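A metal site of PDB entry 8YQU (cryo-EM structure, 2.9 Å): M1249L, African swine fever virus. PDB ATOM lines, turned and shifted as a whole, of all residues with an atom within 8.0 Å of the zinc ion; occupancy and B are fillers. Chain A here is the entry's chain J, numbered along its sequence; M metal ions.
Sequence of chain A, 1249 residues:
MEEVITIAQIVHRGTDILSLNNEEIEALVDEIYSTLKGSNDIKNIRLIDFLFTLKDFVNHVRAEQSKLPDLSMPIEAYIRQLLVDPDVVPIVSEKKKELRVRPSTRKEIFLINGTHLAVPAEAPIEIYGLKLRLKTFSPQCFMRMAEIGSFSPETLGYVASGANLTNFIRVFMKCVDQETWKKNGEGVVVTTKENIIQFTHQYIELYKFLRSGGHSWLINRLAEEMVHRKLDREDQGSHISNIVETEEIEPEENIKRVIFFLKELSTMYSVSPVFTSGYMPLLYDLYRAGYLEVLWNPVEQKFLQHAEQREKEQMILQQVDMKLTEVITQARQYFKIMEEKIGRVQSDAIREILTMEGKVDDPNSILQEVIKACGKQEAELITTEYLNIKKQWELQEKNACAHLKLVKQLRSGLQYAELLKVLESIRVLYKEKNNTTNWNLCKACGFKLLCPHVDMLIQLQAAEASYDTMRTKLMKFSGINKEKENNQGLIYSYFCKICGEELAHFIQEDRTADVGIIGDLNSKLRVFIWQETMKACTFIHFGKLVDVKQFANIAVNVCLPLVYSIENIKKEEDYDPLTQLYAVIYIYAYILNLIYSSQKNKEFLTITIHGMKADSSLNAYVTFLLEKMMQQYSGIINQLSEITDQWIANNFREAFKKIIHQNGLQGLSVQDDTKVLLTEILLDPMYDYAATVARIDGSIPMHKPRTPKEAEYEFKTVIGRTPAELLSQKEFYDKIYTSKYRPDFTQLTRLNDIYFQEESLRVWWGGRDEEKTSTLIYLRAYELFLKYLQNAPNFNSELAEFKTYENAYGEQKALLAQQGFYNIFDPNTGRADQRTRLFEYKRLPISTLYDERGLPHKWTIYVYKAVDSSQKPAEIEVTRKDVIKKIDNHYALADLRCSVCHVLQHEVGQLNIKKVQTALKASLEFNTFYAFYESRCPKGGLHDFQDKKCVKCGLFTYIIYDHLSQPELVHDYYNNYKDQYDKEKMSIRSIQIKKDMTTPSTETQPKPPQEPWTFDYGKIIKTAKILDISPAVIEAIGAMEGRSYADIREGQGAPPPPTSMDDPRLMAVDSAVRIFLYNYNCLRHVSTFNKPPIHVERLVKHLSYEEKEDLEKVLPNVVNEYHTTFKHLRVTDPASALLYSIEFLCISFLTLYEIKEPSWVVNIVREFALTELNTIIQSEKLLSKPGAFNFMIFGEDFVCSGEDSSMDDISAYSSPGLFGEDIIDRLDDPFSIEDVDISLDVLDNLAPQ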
ATOM      1  N   ASN A 399      24.853 -19.767  20.137  1.00  0.00           N
ATOM      2  CA  ASN A 399      24.508 -18.511  20.802  1.00  0.00           C
ATOM      3  C   ASN A 399      23.766 -18.755  22.101  1.00  0.00           C
ATOM      4  O   ASN A 399      22.849 -19.582  22.171  1.00  0.00           O
ATOM      5  CB  ASN A 399      23.667 -17.643  19.864  1.00  0.00           C
ATOM      6  CG  ASN A 399      23.776 -16.168  20.187  1.00  0.00           C
ATOM      7  OD1 ASN A 399      24.313 -15.793  21.233  1.00  0.00           O
ATOM      8  ND2 ASN A 399      23.274 -15.321  19.302  1.00  0.00           N
ATOM      9  N   ALA A 400      24.168 -18.025  23.139  1.00  0.00           N
ATOM     10  CA  ALA A 400      23.486 -18.015  24.428  1.00  0.00           C
ATOM     11  C   ALA A 400      23.315 -16.593  24.939  1.00  0.00           C
ATOM     12  O   ALA A 400      23.349 -16.348  26.147  1.00  0.00           O
ATOM     13  CB  ALA A 400      24.246 -18.870  25.453  1.00  0.00           C
ATOM     14  N   CYS A 401      23.116 -15.643  24.017  1.00  0.00           N
ATOM     15  CA  CYS A 401      23.030 -14.242  24.379  1.00  0.00           C
ATOM     16  C   CYS A 401      21.731 -13.959  25.139  1.00  0.00           C
ATOM     17  O   CYS A 401      20.756 -14.707  25.068  1.00  0.00           O
ATOM     18  CB  CYS A 401      23.104 -13.363  23.121  1.00  0.00           C
ATOM     19  SG  CYS A 401      22.742 -11.616  23.405  1.00  0.00           S
ATOM     20  N   ALA A 402      21.753 -12.853  25.888  1.00  0.00           N
ATOM     21  CA  ALA A 402      20.579 -12.464  26.664  1.00  0.00           C
ATOM     22  C   ALA A 402      19.382 -12.170  25.779  1.00  0.00           C
ATOM     23  O   ALA A 402      18.270 -12.629  26.048  1.00  0.00           O
ATOM     24  CB  ALA A 402      20.912 -11.243  27.537  1.00  0.00           C
ATOM     25  N   HIS A 403      19.614 -11.442  24.670  1.00  0.00           N
ATOM     26  CA  HIS A 403      18.521 -10.957  23.839  1.00  0.00           C
ATOM     27  C   HIS A 403      17.556 -12.081  23.463  1.00  0.00           C
ATOM     28  O   HIS A 403      16.343 -11.882  23.418  1.00  0.00           O
ATOM     29  CB  HIS A 403      19.076 -10.288  22.581  1.00  0.00           C
ATOM     30  CG  HIS A 403      19.440 -11.254  21.490  1.00  0.00           C
ATOM     31  ND1 HIS A 403      20.591 -12.011  21.516  1.00  0.00           N
ATOM     32  CD2 HIS A 403      18.789 -11.601  20.353  1.00  0.00           C
ATOM     33  CE1 HIS A 403      20.650 -12.772  20.441  1.00  0.00           C
ATOM     34  NE2 HIS A 403      19.568 -12.539  19.714  1.00  0.00           N
ATOM     35  N   LEU A 404      18.093 -13.284  23.229  1.00  0.00           N
ATOM     36  CA  LEU A 404      17.268 -14.404  22.812  1.00  0.00           C
ATOM     37  C   LEU A 404      16.105 -14.608  23.773  1.00  0.00           C
ATOM     38  O   LEU A 404      14.939 -14.616  23.340  1.00  0.00           O
ATOM     39  CB  LEU A 404      18.122 -15.678  22.730  1.00  0.00           C
ATOM     40  CG  LEU A 404      19.144 -15.744  21.593  1.00  0.00           C
ATOM     41  CD1 LEU A 404      20.180 -16.827  21.870  1.00  0.00           C
ATOM     42  CD2 LEU A 404      18.456 -15.983  20.264  1.00  0.00           C
ATOM     43  N   LEU A 429      19.205  -2.444  22.021  1.00  0.00           N
ATOM     44  CA  LEU A 429      20.259  -3.256  21.428  1.00  0.00           C
ATOM     45  C   LEU A 429      20.361  -3.096  19.913  1.00  0.00           C
ATOM     46  O   LEU A 429      21.169  -3.795  19.286  1.00  0.00           O
ATOM     47  CB  LEU A 429      20.049  -4.720  21.788  1.00  0.00           C
ATOM     48  CG  LEU A 429      20.191  -5.081  23.273  1.00  0.00           C
ATOM     49  CD1 LEU A 429      19.866  -6.548  23.500  1.00  0.00           C
ATOM     50  CD2 LEU A 429      21.580  -4.754  23.768  1.00  0.00           C
ATOM     51  N   LEU A 441      20.236  -6.111  14.124  1.00  0.00           N
ATOM     52  CA  LEU A 441      21.333  -6.929  14.603  1.00  0.00           C
ATOM     53  C   LEU A 441      21.632  -6.596  16.067  1.00  0.00           C
ATOM     54  O   LEU A 441      21.490  -5.452  16.499  1.00  0.00           O
ATOM     55  CB  LEU A 441      22.590  -6.718  13.756  1.00  0.00           C
ATOM     56  CG  LEU A 441      22.735  -7.507  12.451  1.00  0.00           C
ATOM     57  CD1 LEU A 441      22.807  -9.005  12.716  1.00  0.00           C
ATOM     58  CD2 LEU A 441      21.636  -7.186  11.449  1.00  0.00           C
ATOM     59  N   CYS A 442      22.036  -7.621  16.818  1.00  0.00           N
ATOM     60  CA  CYS A 442      22.326  -7.468  18.242  1.00  0.00           C
ATOM     61  C   CYS A 442      23.765  -7.004  18.411  1.00  0.00           C
ATOM     62  O   CYS A 442      24.696  -7.686  17.986  1.00  0.00           O
ATOM     63  CB  CYS A 442      22.078  -8.779  18.975  1.00  0.00           C
ATOM     64  SG  CYS A 442      22.001  -8.629  20.769  1.00  0.00           S
ATOM     65  N   LYS A 443      23.943  -5.832  19.041  1.00  0.00           N
ATOM     66  CA  LYS A 443      25.292  -5.342  19.288  1.00  0.00           C
ATOM     67  C   LYS A 443      26.030  -6.203  20.315  1.00  0.00           C
ATOM     68  O   LYS A 443      27.254  -6.309  20.275  1.00  0.00           O
ATOM     69  CB  LYS A 443      25.257  -3.885  19.761  1.00  0.00           C
ATOM     70  CG  LYS A 443      24.568  -3.682  21.102  1.00  0.00           C
ATOM     71  CD  LYS A 443      24.631  -2.222  21.517  1.00  0.00           C
ATOM     72  CE  LYS A 443      23.685  -1.369  20.697  1.00  0.00           C
ATOM     73  NZ  LYS A 443      23.631   0.041  21.178  1.00  0.00           N
ATOM     74  N   ALA A 444      25.290  -6.829  21.238  1.00  0.00           N
ATOM     75  CA  ALA A 444      25.919  -7.627  22.277  1.00  0.00           C
ATOM     76  C   ALA A 444      26.558  -8.899  21.739  1.00  0.00           C
ATOM     77  O   ALA A 444      27.616  -9.299  22.216  1.00  0.00           O
ATOM     78  CB  ALA A 444      24.891  -7.977  23.360  1.00  0.00           C
ATOM     79  N   CYS A 445      25.933  -9.533  20.744  1.00  0.00           N
ATOM     80  CA  CYS A 445      26.442 -10.788  20.197  1.00  0.00           C
ATOM     81  C   CYS A 445      26.860 -10.665  18.745  1.00  0.00           C
ATOM     82  O   CYS A 445      27.999 -11.005  18.396  1.00  0.00           O
ATOM     83  CB  CYS A 445      25.394 -11.899  20.361  1.00  0.00           C
ATOM     84  SG  CYS A 445      25.962 -13.511  19.788  1.00  0.00           S
ATOM     85  N   GLY A 446      25.979 -10.180  17.878  1.00  0.00           N
ATOM     86  CA  GLY A 446      26.265 -10.012  16.459  1.00  0.00           C
ATOM     87  C   GLY A 446      25.275 -10.656  15.522  1.00  0.00           C
ATOM     88  O   GLY A 446      25.299 -10.362  14.322  1.00  0.00           O
ATOM     89  N   PHE A 447      24.406 -11.533  16.018  1.00  0.00           N
ATOM     90  CA  PHE A 447      23.428 -12.204  15.168  1.00  0.00           C
ATOM     91  C   PHE A 447      22.131 -11.395  15.105  1.00  0.00           C
ATOM     92  O   PHE A 447      21.999 -10.333  15.712  1.00  0.00           O
ATOM     93  CB  PHE A 447      23.167 -13.624  15.665  1.00  0.00           C
ATOM     94  CG  PHE A 447      24.373 -14.521  15.588  1.00  0.00           C
ATOM     95  CD1 PHE A 447      24.758 -15.077  14.380  1.00  0.00           C
ATOM     96  CD2 PHE A 447      25.124 -14.796  16.710  1.00  0.00           C
ATOM     97  CE1 PHE A 447      25.865 -15.902  14.295  1.00  0.00           C
ATOM     98  CE2 PHE A 447      26.234 -15.613  16.645  1.00  0.00           C
ATOM     99  CZ  PHE A 447      26.610 -16.166  15.438  1.00  0.00           C
ATOM    100  N   LYS A 448      21.162 -11.909  14.345  1.00  0.00           N
ATOM    101  CA  LYS A 448      19.914 -11.195  14.132  1.00  0.00           C
ATOM    102  C   LYS A 448      19.151 -11.036  15.436  1.00  0.00           C
ATOM    103  O   LYS A 448      19.162 -11.925  16.296  1.00  0.00           O
ATOM    104  CB  LYS A 448      19.060 -11.934  13.098  1.00  0.00           C
ATOM    105  CG  LYS A 448      19.679 -11.957  11.703  1.00  0.00           C
ATOM    106  CD  LYS A 448      18.878 -12.824  10.757  1.00  0.00           C
ATOM    107  CE  LYS A 448      19.604 -13.016   9.444  1.00  0.00           C
ATOM    108  NZ  LYS A 448      19.904 -11.729   8.765  1.00  0.00           N
ATOM    109  N   LEU A 449      18.460  -9.900  15.578  1.00  0.00           N
ATOM    110  CA  LEU A 449      17.778  -9.561  16.817  1.00  0.00           C
ATOM    111  C   LEU A 449      16.255  -9.528  16.654  1.00  0.00           C
ATOM    112  O   LEU A 449      15.543 -10.233  17.380  1.00  0.00           O
ATOM    113  CB  LEU A 449      18.288  -8.217  17.341  1.00  0.00           C
ATOM    114  CG  LEU A 449      17.569  -7.583  18.540  1.00  0.00           C
ATOM    115  CD1 LEU A 449      17.546  -8.530  19.720  1.00  0.00           C
ATOM    116  CD2 LEU A 449      18.244  -6.276  18.919  1.00  0.00           C
HETATM  117 ZN    ZN M   1      22.538 -10.814  21.259  1.00  0.00          ZN
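CB of Cys 445 touches the zinc ion, at 3.2 Å.
Of the 16 residues printed, 4 come within 4 Å of the zinc ion.
The nearest printed residue that does not touch the zinc ion is Ala 444 (4.2 Å).
A ring nitrogen (NE2) of His 403 sits at hydrogen-bond distance from the backbone carbonyl oxygen of Lys 448 (3.5 Å).
The backbone NH of Cys 401 lies within hydrogen-bond range of the side-chain amide oxygen of Asn 399.
The backbone NH (N) of Ala 444 lies close to the side-chain sulfur (SG) of Cys 442, at 3.8 Å.
The backbone NH of Cys 442 sits at hydrogen-bond distance from the backbone carbonyl oxygen of Phe 447.
OD1 of Asn 399 sits at hydrogen-bond distance from SG of Cys 445.
The zinc ion is bound by a ring nitrogen (ND1) of His 403 (2.3 Å), the side-chain sulfur of Cys 401 (2.3 Å) and the side-chain sulfur of Cys 442 (2.3 Å).
The zinc ion has three donor atoms within binding distance.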
